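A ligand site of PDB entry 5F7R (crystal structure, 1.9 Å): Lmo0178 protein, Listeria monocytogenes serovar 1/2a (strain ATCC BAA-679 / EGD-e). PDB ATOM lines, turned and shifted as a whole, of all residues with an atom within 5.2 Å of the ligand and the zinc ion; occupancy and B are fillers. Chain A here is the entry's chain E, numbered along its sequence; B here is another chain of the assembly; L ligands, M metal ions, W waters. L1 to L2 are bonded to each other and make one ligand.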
ATOM      1  N   LYS A  89      -8.860 -23.741   6.923  1.00  0.00           N
ATOM      2  CA  LYS A  89      -9.762 -23.516   5.791  1.00  0.00           C
ATOM      3  C   LYS A  89      -9.565 -22.087   5.314  1.00  0.00           C
ATOM      4  O   LYS A  89      -9.731 -21.155   6.076  1.00  0.00           O
ATOM      5  CB  LYS A  89     -11.219 -23.750   6.164  1.00  0.00           C
ATOM      6  CG  LYS A  89     -12.143 -23.706   4.946  1.00  0.00           C
ATOM      7  CD  LYS A  89     -13.606 -23.594   5.332  1.00  0.00           C
ATOM      8  CE  LYS A  89     -14.498 -23.718   4.096  1.00  0.00           C
ATOM      9  NZ  LYS A  89     -15.889 -23.276   4.318  1.00  0.00           N
ATOM     10  N   VAL A  90      -9.185 -21.951   4.049  1.00  0.00           N
ATOM     11  CA  VAL A  90      -8.968 -20.642   3.466  1.00  0.00           C
ATOM     12  C   VAL A  90     -10.282 -20.220   2.792  1.00  0.00           C
ATOM     13  O   VAL A  90     -10.585 -20.712   1.710  1.00  0.00           O
ATOM     14  CB  VAL A  90      -7.831 -20.673   2.441  1.00  0.00           C
ATOM     15  CG1 VAL A  90      -7.628 -19.281   1.822  1.00  0.00           C
ATOM     16  CG2 VAL A  90      -6.562 -21.166   3.102  1.00  0.00           C
ATOM     17  N   GLU A  91     -11.054 -19.384   3.467  1.00  0.00           N
ATOM     18  CA  GLU A  91     -12.219 -18.747   2.866  1.00  0.00           C
ATOM     19  C   GLU A  91     -11.803 -17.412   2.291  1.00  0.00           C
ATOM     20  O   GLU A  91     -10.650 -17.007   2.388  1.00  0.00           O
ATOM     21  CB  GLU A  91     -13.336 -18.592   3.879  1.00  0.00           C
ATOM     22  CG  GLU A  91     -13.838 -19.903   4.468  1.00  0.00           C
ATOM     23  CD  GLU A  91     -15.070 -19.754   5.353  1.00  0.00           C
ATOM     24  OE1 GLU A  91     -15.757 -20.761   5.641  1.00  0.00           O
ATOM     25  OE2 GLU A  91     -15.320 -18.644   5.840  1.00  0.00           O
ATOM     26  N   GLU A  92     -12.733 -16.699   1.675  1.00  0.00           N
ATOM     27  CA  GLU A  92     -12.335 -15.539   0.922  1.00  0.00           C
ATOM     28  C   GLU A  92     -12.133 -14.332   1.841  1.00  0.00           C
ATOM     29  O   GLU A  92     -11.278 -13.476   1.576  1.00  0.00           O
ATOM     30  CB  GLU A  92     -13.334 -15.263  -0.208  1.00  0.00           C
ATOM     31  CG  GLU A  92     -13.390 -16.416  -1.227  1.00  0.00           C
ATOM     32  CD  GLU A  92     -14.246 -17.603  -0.757  1.00  0.00           C
ATOM     33  OE1 GLU A  92     -15.349 -17.363  -0.214  1.00  0.00           O
ATOM     34  OE2 GLU A  92     -13.838 -18.771  -0.948  1.00  0.00           O
ATOM     35  N   SER A 151     -10.448 -23.301  -1.935  1.00  0.00           N
ATOM     36  CA  SER A 151     -11.208 -23.260  -3.194  1.00  0.00           C
ATOM     37  C   SER A 151     -10.290 -23.482  -4.409  1.00  0.00           C
ATOM     38  O   SER A 151      -9.111 -23.160  -4.363  1.00  0.00           O
ATOM     39  CB  SER A 151     -11.872 -21.893  -3.314  1.00  0.00           C
ATOM     40  OG  SER A 151     -10.920 -20.857  -3.224  1.00  0.00           O
ATOM     41  N   GLY A 152     -10.832 -24.048  -5.467  1.00  0.00           N
ATOM     42  CA  GLY A 152     -10.170 -24.022  -6.766  1.00  0.00           C
ATOM     43  C   GLY A 152      -9.498 -25.321  -7.139  1.00  0.00           C
ATOM     44  O   GLY A 152      -9.714 -26.374  -6.534  1.00  0.00           O
ATOM     45  N   LEU A 153      -8.708 -25.239  -8.206  1.00  0.00           N
ATOM     46  CA  LEU A 153      -7.936 -26.365  -8.718  1.00  0.00           C
ATOM     47  C   LEU A 153      -6.636 -26.492  -7.908  1.00  0.00           C
ATOM     48  O   LEU A 153      -5.792 -25.580  -7.883  1.00  0.00           O
ATOM     49  CB  LEU A 153      -7.635 -26.140 -10.202  1.00  0.00           C
ATOM     50  CG  LEU A 153      -6.769 -27.217 -10.844  1.00  0.00           C
ATOM     51  CD1 LEU A 153      -7.466 -28.579 -10.789  1.00  0.00           C
ATOM     52  CD2 LEU A 153      -6.408 -26.845 -12.273  1.00  0.00           C
ATOM     53  N   THR A 165     -10.084 -19.004  -8.700  1.00  0.00           N
ATOM     54  CA  THR A 165     -10.683 -17.760  -9.113  1.00  0.00           C
ATOM     55  C   THR A 165     -11.516 -17.163  -7.979  1.00  0.00           C
ATOM     56  O   THR A 165     -11.824 -15.990  -8.012  1.00  0.00           O
ATOM     57  CB  THR A 165     -11.513 -17.935 -10.373  1.00  0.00           C
ATOM     58  OG1 THR A 165     -12.574 -18.863 -10.125  1.00  0.00           O
ATOM     59  CG2 THR A 165     -10.635 -18.438 -11.486  1.00  0.00           C
ATOM     60  N   MET A 166     -11.861 -17.957  -6.968  1.00  0.00           N
ATOM     61  CA  MET A 166     -12.503 -17.390  -5.760  1.00  0.00           C
ATOM     62  C   MET A 166     -11.555 -16.430  -5.054  1.00  0.00           C
ATOM     63  O   MET A 166     -12.001 -15.444  -4.471  1.00  0.00           O
ATOM     64  CB  MET A 166     -12.894 -18.483  -4.755  1.00  0.00           C
ATOM     65  CG  MET A 166     -14.082 -19.297  -5.161  1.00  0.00           C
ATOM     66  SD  MET A 166     -15.616 -18.357  -5.156  1.00  0.00           S
ATOM     67  CE  MET A 166     -15.951 -18.200  -3.435  1.00  0.00           C
ATOM     68  N   LYS A 191      -9.139 -29.546  -2.271  1.00  0.00           N
ATOM     69  CA  LYS A 191     -10.308 -28.681  -2.445  1.00  0.00           C
ATOM     70  C   LYS A 191     -11.239 -28.762  -1.228  1.00  0.00           C
ATOM     71  O   LYS A 191     -11.491 -29.834  -0.676  1.00  0.00           O
ATOM     72  CB  LYS A 191     -11.045 -29.038  -3.721  1.00  0.00           C
ATOM     73  CG  LYS A 191     -12.184 -28.069  -4.063  1.00  0.00           C
ATOM     74  CD  LYS A 191     -12.770 -28.344  -5.417  1.00  0.00           C
ATOM     75  CE  LYS A 191     -13.363 -29.725  -5.521  1.00  0.00           C
ATOM     76  NZ  LYS A 191     -14.202 -29.842  -6.751  1.00  0.00           N
ATOM     77  N   ASN A 192     -11.750 -27.588  -0.851  1.00  0.00           N
ATOM     78  CA  ASN A 192     -12.572 -27.427   0.326  1.00  0.00           C
ATOM     79  C   ASN A 192     -13.666 -28.496   0.488  1.00  0.00           C
ATOM     80  O   ASN A 192     -13.693 -29.200   1.496  1.00  0.00           O
ATOM     81  CB  ASN A 192     -13.138 -25.995   0.442  1.00  0.00           C
ATOM     82  CG  ASN A 192     -13.791 -25.486  -0.832  1.00  0.00           C
ATOM     83  OD1 ASN A 192     -14.356 -26.246  -1.629  1.00  0.00           O
ATOM     84  ND2 ASN A 192     -13.769 -24.174  -1.000  1.00  0.00           N
ATOM     85  N   ILE A 193     -14.444 -28.715  -0.567  1.00  0.00           N
ATOM     86  CA  ILE A 193     -15.579 -29.619  -0.474  1.00  0.00           C
ATOM     87  C   ILE A 193     -15.119 -31.087  -0.445  1.00  0.00           C
ATOM     88  O   ILE A 193     -15.783 -31.947   0.113  1.00  0.00           O
ATOM     89  CB  ILE A 193     -16.620 -29.331  -1.619  1.00  0.00           C
ATOM     90  CG1 ILE A 193     -17.864 -30.195  -1.517  1.00  0.00           C
ATOM     91  CG2 ILE A 193     -16.021 -29.581  -2.986  1.00  0.00           C
ATOM     92  CD1 ILE A 193     -18.561 -30.136  -0.197  1.00  0.00           C
ATOM     93  N   SER A 216     -22.256 -28.234  -1.741  1.00  0.00           N
ATOM     94  CA  SER A 216     -22.157 -27.164  -0.739  1.00  0.00           C
ATOM     95  C   SER A 216     -22.826 -25.914  -1.219  1.00  0.00           C
ATOM     96  O   SER A 216     -22.668 -25.534  -2.369  1.00  0.00           O
ATOM     97  CB  SER A 216     -20.707 -26.890  -0.331  1.00  0.00           C
ATOM     98  OG  SER A 216     -19.945 -26.362  -1.394  1.00  0.00           O
ATOM     99  N   VAL A 217     -23.534 -25.273  -0.290  1.00  0.00           N
ATOM    100  CA  VAL A 217     -24.248 -24.029  -0.535  1.00  0.00           C
ATOM    101  C   VAL A 217     -23.695 -22.960   0.409  1.00  0.00           C
ATOM    102  O   VAL A 217     -23.436 -23.227   1.600  1.00  0.00           O
ATOM    103  CB  VAL A 217     -25.773 -24.201  -0.368  1.00  0.00           C
ATOM    104  CG1 VAL A 217     -26.147 -24.775   0.972  1.00  0.00           C
ATOM    105  CG2 VAL A 217     -26.506 -22.890  -0.591  1.00  0.00           C
ATOM    106  N   GLY A 218     -23.512 -21.748  -0.129  1.00  0.00           N
ATOM    107  CA  GLY A 218     -22.942 -20.646   0.619  1.00  0.00           C
ATOM    108  C   GLY A 218     -22.276 -19.697  -0.346  1.00  0.00           C
ATOM    109  O   GLY A 218     -22.927 -19.215  -1.294  1.00  0.00           O
ATOM    110  N   ALA A 219     -21.009 -19.359  -0.085  1.00  0.00           N
ATOM    111  CA  ALA A 219     -20.312 -18.337  -0.867  1.00  0.00           C
ATOM    112  C   ALA A 219     -20.215 -18.719  -2.345  1.00  0.00           C
ATOM    113  O   ALA A 219     -20.411 -17.873  -3.231  1.00  0.00           O
ATOM    114  CB  ALA A 219     -18.912 -18.107  -0.327  1.00  0.00           C
ATOM    115  N   GLY A 220     -19.875 -19.980  -2.583  1.00  0.00           N
ATOM    116  CA  GLY A 220     -19.936 -20.579  -3.902  1.00  0.00           C
ATOM    117  C   GLY A 220     -20.730 -21.862  -3.861  1.00  0.00           C
ATOM    118  O   GLY A 220     -21.365 -22.176  -2.834  1.00  0.00           O
ATOM    119  N   LEU A 221     -20.722 -22.574  -4.974  1.00  0.00           N
ATOM    120  CA  LEU A 221     -21.321 -23.888  -5.058  1.00  0.00           C
ATOM    121  C   LEU A 221     -20.246 -24.944  -5.365  1.00  0.00           C
ATOM    122  O   LEU A 221     -19.520 -24.874  -6.373  1.00  0.00           O
ATOM    123  CB  LEU A 221     -22.392 -23.874  -6.121  1.00  0.00           C
ATOM    124  CG  LEU A 221     -23.392 -25.032  -6.064  1.00  0.00           C
ATOM    125  CD1 LEU A 221     -24.627 -24.687  -6.864  1.00  0.00           C
ATOM    126  CD2 LEU A 221     -22.788 -26.315  -6.577  1.00  0.00           C
ATOM    127  N   GLY A 222     -20.154 -25.927  -4.481  1.00  0.00           N
ATOM    128  CA  GLY A 222     -19.163 -26.988  -4.613  1.00  0.00           C
ATOM    129  C   GLY A 222     -19.816 -28.339  -4.771  1.00  0.00           C
ATOM    130  O   GLY A 222     -20.967 -28.535  -4.397  1.00  0.00           O
ATOM    131  N   LEU A 223     -19.049 -29.282  -5.298  1.00  0.00           N
ATOM    132  CA  LEU A 223     -19.485 -30.659  -5.496  1.00  0.00           C
ATOM    133  C   LEU A 223     -18.331 -31.596  -5.199  1.00  0.00           C
ATOM    134  O   LEU A 223     -17.224 -31.399  -5.705  1.00  0.00           O
ATOM    135  CB  LEU A 223     -19.964 -30.902  -6.934  1.00  0.00           C
ATOM    136  CG  LEU A 223     -20.279 -32.341  -7.344  1.00  0.00           C
ATOM    137  CD1 LEU A 223     -21.509 -32.843  -6.593  1.00  0.00           C
ATOM    138  CD2 LEU A 223     -20.503 -32.514  -8.831  1.00  0.00           C
ATOM    139  N   GLU A 241     -16.061 -29.194 -10.437  1.00  0.00           N
ATOM    140  CA  GLU A 241     -16.274 -27.748 -10.584  1.00  0.00           C
ATOM    141  C   GLU A 241     -17.638 -27.458 -11.143  1.00  0.00           C
ATOM    142  O   GLU A 241     -17.822 -26.702 -12.134  1.00  0.00           O
ATOM    143  CB  GLU A 241     -15.163 -27.049 -11.362  1.00  0.00           C
ATOM    144  CG  GLU A 241     -13.851 -26.938 -10.604  1.00  0.00           C
ATOM    145  CD  GLU A 241     -13.927 -26.069  -9.337  1.00  0.00           C
ATOM    146  OE1 GLU A 241     -14.728 -25.101  -9.250  1.00  0.00           O
ATOM    147  OE2 GLU A 241     -13.161 -26.370  -8.390  1.00  0.00           O
ATOM    148  N   GLY A 243     -19.960 -25.680  -9.905  1.00  0.00           N
ATOM    149  CA  GLY A 243     -20.281 -24.260  -9.864  1.00  0.00           C
ATOM    150  C   GLY A 243     -20.056 -23.554 -11.190  1.00  0.00           C
ATOM    151  O   GLY A 243     -20.654 -22.497 -11.448  1.00  0.00           O
ATOM    152  N   HIS A 244     -19.182 -24.115 -12.011  1.00  0.00           N
ATOM    153  CA  HIS A 244     -18.848 -23.524 -13.308  1.00  0.00           C
ATOM    154  C   HIS A 244     -19.363 -24.333 -14.469  1.00  0.00           C
ATOM    155  O   HIS A 244     -18.833 -24.250 -15.574  1.00  0.00           O
ATOM    156  CB  HIS A 244     -17.336 -23.303 -13.326  1.00  0.00           C
ATOM    157  CG  HIS A 244     -16.901 -22.550 -12.143  1.00  0.00           C
ATOM    158  ND1 HIS A 244     -17.230 -21.214 -11.984  1.00  0.00           N
ATOM    159  CD2 HIS A 244     -16.481 -22.979 -10.931  1.00  0.00           C
ATOM    160  CE1 HIS A 244     -16.957 -20.850 -10.741  1.00  0.00           C
ATOM    161  NE2 HIS A 244     -16.433 -21.879 -10.108  1.00  0.00           N
ATOM    162  N   CYS A 254     -18.820 -14.652 -14.672  1.00  0.00           N
ATOM    163  CA  CYS A 254     -18.271 -15.300 -13.481  1.00  0.00           C
ATOM    164  C   CYS A 254     -16.804 -14.899 -13.230  1.00  0.00           C
ATOM    165  O   CYS A 254     -16.085 -14.570 -14.162  1.00  0.00           O
ATOM    166  CB  CYS A 254     -18.387 -16.824 -13.636  1.00  0.00           C
ATOM    167  SG  CYS A 254     -17.900 -17.831 -12.201  1.00  0.00           S
ATOM    168  N   HIS A 255     -16.353 -15.066 -11.990  1.00  0.00           N
ATOM    169  CA  HIS A 255     -14.934 -14.915 -11.636  1.00  0.00           C
ATOM    170  C   HIS A 255     -14.011 -15.870 -12.398  1.00  0.00           C
ATOM    171  O   HIS A 255     -12.833 -15.558 -12.623  1.00  0.00           O
ATOM    172  CB  HIS A 255     -14.699 -15.009 -10.103  1.00  0.00           C
ATOM    173  CG  HIS A 255     -15.360 -16.199  -9.455  1.00  0.00           C
ATOM    174  ND1 HIS A 255     -14.781 -17.436  -9.435  1.00  0.00           N
ATOM    175  CD2 HIS A 255     -16.561 -16.330  -8.852  1.00  0.00           C
ATOM    176  CE1 HIS A 255     -15.575 -18.284  -8.816  1.00  0.00           C
ATOM    177  NE2 HIS A 255     -16.669 -17.646  -8.463  1.00  0.00           N
ATOM    178  N   CYS A 256     -14.569 -16.985 -12.887  1.00  0.00           N
ATOM    179  CA  CYS A 256     -13.789 -17.941 -13.664  1.00  0.00           C
ATOM    180  C   CYS A 256     -13.560 -17.490 -15.128  1.00  0.00           C
ATOM    181  O   CYS A 256     -12.832 -18.147 -15.852  1.00  0.00           O
ATOM    182  CB  CYS A 256     -14.426 -19.330 -13.579  1.00  0.00           C
ATOM    183  SG  CYS A 256     -15.782 -19.613 -14.769  1.00  0.00           S
ATOM    184  N   GLN A 258     -15.983 -17.316 -17.477  1.00  0.00           N
ATOM    185  CA  GLN A 258     -17.161 -17.769 -18.290  1.00  0.00           C
ATOM    186  C   GLN A 258     -18.389 -16.870 -18.033  1.00  0.00           C
ATOM    187  O   GLN A 258     -18.369 -16.066 -17.098  1.00  0.00           O
ATOM    188  CB  GLN A 258     -17.525 -19.240 -17.977  1.00  0.00           C
ATOM    189  CG  GLN A 258     -16.383 -20.234 -18.161  1.00  0.00           C
ATOM    190  CD  GLN A 258     -16.655 -21.649 -17.638  1.00  0.00           C
ATOM    191  OE1 GLN A 258     -15.730 -22.474 -17.596  1.00  0.00           O
ATOM    192  NE2 GLN A 258     -17.913 -21.955 -17.273  1.00  0.00           N
ATOM    193  N   CYS A 261     -22.413 -19.225 -15.378  1.00  0.00           N
ATOM    194  CA  CYS A 261     -22.124 -20.310 -14.461  1.00  0.00           C
ATOM    195  C   CYS A 261     -23.190 -20.452 -13.373  1.00  0.00           C
ATOM    196  O   CYS A 261     -23.728 -19.464 -12.859  1.00  0.00           O
ATOM    197  CB  CYS A 261     -20.783 -20.084 -13.790  1.00  0.00           C
ATOM    198  SG  CYS A 261     -19.403 -20.112 -14.917  1.00  0.00           S
ATOM    199  N   GLU A 263     -22.921 -21.124 -10.346  1.00  0.00           N
ATOM    200  CA  GLU A 263     -22.542 -20.401  -9.132  1.00  0.00           C
ATOM    201  C   GLU A 263     -22.975 -18.936  -9.144  1.00  0.00           C
ATOM    202  O   GLU A 263     -23.135 -18.311  -8.094  1.00  0.00           O
ATOM    203  CB  GLU A 263     -21.028 -20.523  -8.988  1.00  0.00           C
ATOM    204  CG  GLU A 263     -20.397 -19.836  -7.828  1.00  0.00           C
ATOM    205  CD  GLU A 263     -19.066 -20.470  -7.530  1.00  0.00           C
ATOM    206  OE1 GLU A 263     -18.043 -19.793  -7.800  1.00  0.00           O
ATOM    207  OE2 GLU A 263     -19.063 -21.665  -7.167  1.00  0.00           O
ATOM    208  N   GLY A 337     -22.811 -26.937   3.972  1.00  0.00           N
ATOM    209  CA  GLY A 337     -22.285 -25.603   3.772  1.00  0.00           C
ATOM    210  C   GLY A 337     -22.920 -24.533   4.638  1.00  0.00           C
ATOM    211  O   GLY A 337     -23.968 -24.740   5.277  1.00  0.00           O
ATOM    212  N   GLU A 338     -22.290 -23.369   4.652  1.00  0.00           N
ATOM    213  CA  GLU A 338     -22.696 -22.300   5.526  1.00  0.00           C
ATOM    214  C   GLU A 338     -24.044 -21.718   5.157  1.00  0.00           C
ATOM    215  O   GLU A 338     -24.713 -21.137   6.002  1.00  0.00           O
ATOM    216  CB  GLU A 338     -21.624 -21.207   5.583  1.00  0.00           C
ATOM    217  CG  GLU A 338     -20.292 -21.679   6.100  1.00  0.00           C
ATOM    218  CD  GLU A 338     -19.414 -22.380   5.061  1.00  0.00           C
ATOM    219  OE1 GLU A 338     -18.368 -22.940   5.457  1.00  0.00           O
ATOM    220  OE2 GLU A 338     -19.759 -22.378   3.857  1.00  0.00           O
ATOM    221  N   TRP A 378     -15.617 -28.784   7.926  1.00  0.00           N
ATOM    222  CA  TRP A 378     -14.666 -28.426   6.880  1.00  0.00           C
ATOM    223  C   TRP A 378     -13.251 -28.619   7.428  1.00  0.00           C
ATOM    224  O   TRP A 378     -12.355 -29.081   6.732  1.00  0.00           O
ATOM    225  CB  TRP A 378     -14.819 -26.981   6.390  1.00  0.00           C
ATOM    226  CG  TRP A 378     -16.138 -26.692   5.727  1.00  0.00           C
ATOM    227  CD1 TRP A 378     -17.311 -26.286   6.338  1.00  0.00           C
ATOM    228  CD2 TRP A 378     -16.420 -26.726   4.321  1.00  0.00           C
ATOM    229  NE1 TRP A 378     -18.311 -26.137   5.398  1.00  0.00           N
ATOM    230  CE2 TRP A 378     -17.789 -26.362   4.158  1.00  0.00           C
ATOM    231  CE3 TRP A 378     -15.682 -27.076   3.176  1.00  0.00           C
ATOM    232  CZ2 TRP A 378     -18.406 -26.333   2.904  1.00  0.00           C
ATOM    233  CZ3 TRP A 378     -16.300 -26.982   1.932  1.00  0.00           C
ATOM    234  CH2 TRP A 378     -17.639 -26.654   1.818  1.00  0.00           C
ATOM    235  N   PHE B 358     -12.706 -24.732 -17.004  1.00  0.00           N
ATOM    236  CA  PHE B 358     -12.085 -24.305 -15.764  1.00  0.00           C
ATOM    237  C   PHE B 358     -10.579 -24.600 -15.757  1.00  0.00           C
ATOM    238  O   PHE B 358      -9.810 -23.825 -15.229  1.00  0.00           O
ATOM    239  CB  PHE B 358     -12.749 -24.938 -14.551  1.00  0.00           C
ATOM    240  CG  PHE B 358     -12.391 -24.249 -13.260  1.00  0.00           C
ATOM    241  CD1 PHE B 358     -13.061 -23.108 -12.855  1.00  0.00           C
ATOM    242  CD2 PHE B 358     -11.301 -24.670 -12.521  1.00  0.00           C
ATOM    243  CE1 PHE B 358     -12.696 -22.433 -11.699  1.00  0.00           C
ATOM    244  CE2 PHE B 358     -10.925 -24.012 -11.355  1.00  0.00           C
ATOM    245  CZ  PHE B 358     -11.634 -22.892 -10.934  1.00  0.00           C
HETATM  246  C1  LIG L   1     -16.010 -22.355  -6.220  1.00  0.00           C
HETATM  247  C2  LIG L   1     -14.653 -23.029  -6.396  1.00  0.00           C
HETATM  248  C3  LIG L   1     -14.729 -24.494  -5.993  1.00  0.00           C
HETATM  249  C4  LIG L   1     -15.257 -24.618  -4.572  1.00  0.00           C
HETATM  250  C5  LIG L   1     -16.617 -23.922  -4.509  1.00  0.00           C
HETATM  251  C6  LIG L   1     -17.275 -24.027  -3.157  1.00  0.00           C
HETATM  252  O1  LIG L   1     -16.912 -22.937  -7.173  1.00  0.00           O
HETATM  253  O2  LIG L   1     -14.233 -22.958  -7.766  1.00  0.00           O
HETATM  254  O3  LIG L   1     -13.414 -25.062  -6.143  1.00  0.00           O
HETATM  255  O4  LIG L   1     -15.435 -25.993  -4.177  1.00  0.00           O
HETATM  256  O5  LIG L   1     -16.484 -22.557  -4.881  1.00  0.00           O
HETATM  257  O6  LIG L   1     -16.478 -23.354  -2.166  1.00  0.00           O
HETATM  258  C1  LG2 L   2     -17.025 -22.072  -1.797  1.00  0.00           C
HETATM  259  C2  LG2 L   2     -16.128 -21.422  -0.742  1.00  0.00           C
HETATM  260  C3  LG2 L   2     -16.199 -22.172   0.580  1.00  0.00           C
HETATM  261  C4  LG2 L   2     -17.654 -22.299   1.004  1.00  0.00           C
HETATM  262  C5  LG2 L   2     -18.473 -22.945  -0.111  1.00  0.00           C
HETATM  263  C6  LG2 L   2     -19.951 -23.108   0.224  1.00  0.00           C
HETATM  264  O1  LG2 L   2     -14.782 -21.372  -1.206  1.00  0.00           O
HETATM  265  O2  LG2 L   2     -15.395 -21.515   1.589  1.00  0.00           O
HETATM  266  O3  LG2 L   2     -17.769 -23.114   2.182  1.00  0.00           O
HETATM  267  O4  LG2 L   2     -18.353 -22.164  -1.302  1.00  0.00           O
HETATM  268  O5  LG2 L   2     -20.635 -23.797  -0.838  1.00  0.00           O
HETATM  269 ZN    ZN M   1     -17.627 -19.786 -13.446  1.00  0.00          ZN
HETATM  270  O   HOH W   1     -12.781 -22.596   1.269  1.00  0.00           O
HETATM  271  O   HOH W   2     -16.333 -27.814  -6.108  1.00  0.00           O
HETATM  272  O   HOH W   3     -12.332 -20.932  -8.028  1.00  0.00           O
HETATM  273  O   HOH W   4     -16.110 -19.008   1.858  1.00  0.00           O
HETATM  274  O   HOH W   5     -17.606 -25.827  -8.124  1.00  0.00           O
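An oxygen (O1) of LIG L1 sits at hydrogen-bond distance from a ring nitrogen (NE2) of His 244, 3.2 Å away.
The side-chain carboxylate of Glu 263 sits at hydrogen-bond distance from an oxygen (O1) of LIG L1 (2.5 Å).
The side-chain carboxylate (OE2) of Glu 241 lies within hydrogen-bond range of an oxygen (O3) of LIG L1 (2.6 Å).
The backbone NH (N) of Gly 220 sits at hydrogen-bond distance from an oxygen (O4) of LG2 L2, 3.0 Å away.
O5 of LG2 L2 sits at hydrogen-bond distance from O of Gly 220 (2.7 Å).
An oxygen (O3) of LG2 L2 sits at hydrogen-bond distance from the side-chain carboxylate (OE2) of Glu 338, 2.7 Å away.
The backbone carbonyl oxygen of Ser 216 lies close to an oxygen (O5) of LG2 L2 (3.1 Å).
An oxygen (O5) of LG2 L2 sits at hydrogen-bond distance from the side-chain hydroxyl of Ser 216, at 2.7 Å.
OD1 of Asn 192 sits at hydrogen-bond distance from O4 of LIG L1, 2.8 Å away.
The side-chain carboxylate (OE2) of Glu 92 lies within hydrogen-bond range of an oxygen (O1) of LG2 L2 (2.8 Å).
An oxygen (O3) of LG2 L2 lies within hydrogen-bond range of the side-chain amino group of Lys 89.
N of Gly 152 sits at hydrogen-bond distance from O3 of LIG L1.
The backbone NH of Val 217 sits at hydrogen-bond distance from an oxygen (O5) of LG2 L2, 3.3 Å away.
The backbone carbonyl oxygen (O) of Leu 221 lies within hydrogen-bond range of an oxygen (O1) of LIG L1 (3.3 Å).
N of Gln 258 sits close to SG of Cys 256, 3.6 Å away.
The side-chain sulfur (SG) of Cys 261 lies close to the side-chain amide nitrogen (NE2) of Gln 258.
The backbone NH of Leu 221 lies within hydrogen-bond range of the side-chain carboxylate of Glu 263 (2.9 Å).
The side-chain carboxylate (OE2) of Glu 241 is in salt-bridge range of the side-chain amino group (NZ) of Lys 191, 3.98 Å away.
The side-chain carboxylate (OE1) of Glu 338 lies within salt-bridge range of the side-chain amino group (NZ) of Lys 89 (2.7 Å).
The backbone NH (N) of Glu 338 sits at hydrogen-bond distance from the backbone carbonyl oxygen (O) of Val 217, 3.3 Å away.
The side-chain carboxylate (OE1) of Glu 338 sits at hydrogen-bond distance from the indole nitrogen (NE1) of Trp 378 (3.2 Å).
NZ of Lys 89 is in salt-bridge range of OE1 of Glu 91.
Residues that only touch the ligand: Trp 378 (3.4 Å), Lys 191 (3.4 Å), Gly 218 (3.6 Å), Ser 151 (3.6 Å), Glu 91 (3.6 Å), Gly 222 (3.7 Å), Met 166 (3.8 Å), Ile 193 (3.8 Å) and Ala 219 (3.9 Å).
Hydrophobic or aromatic side chains that line the ligand: Met 166, Ile 193, His 244 and Trp 378.
Of the 33 residues printed, 21 come within 4 Å of the ligand.
Of the 33 residues printed, 4 come within 4 Å of the zinc ion.
Along chain A the residues within 4 Å of the zinc ion span positions 244 to 261.
The zinc ion is bound by ND1 of His 244 (2.1 Å).
The zinc ion is bound by SG of Cys 256, at 2.3 Å.
SG of Cys 261 binds the zinc ion, at 2.3 Å.
SG of Cys 254 is bound to the zinc ion, at 2.3 Å.
The zinc ion has four donor atoms within binding distance.
Water W4 bridges O2 of LG2 L2 (2.6 Å) and OE1 of Glu 92 (2.8 Å).
Water W3 lies within hydrogen-bond range of O2 of LIG L1 (2.8 Å), OG1 of Thr 165 (3.0 Å) and N of Met 166 (3.2 Å).
Water W2 lies within hydrogen-bond range of O4 of LIG L1 (2.8 Å), NZ of Lys 191 (3.0 Å) and N of Leu 223 (3.2 Å).
Water W1 lies within hydrogen-bond range of an oxygen (O2) of LG2 L2 (2.8 Å), the backbone carbonyl oxygen of Val 90 (2.9 Å) and the side-chain amide nitrogen of Asn 192 (2.9 Å).
Water W5 lies within hydrogen-bond range of O of Leu 221, N of Gly 243, O1 of LIG L1 and OE1 of Glu 241.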
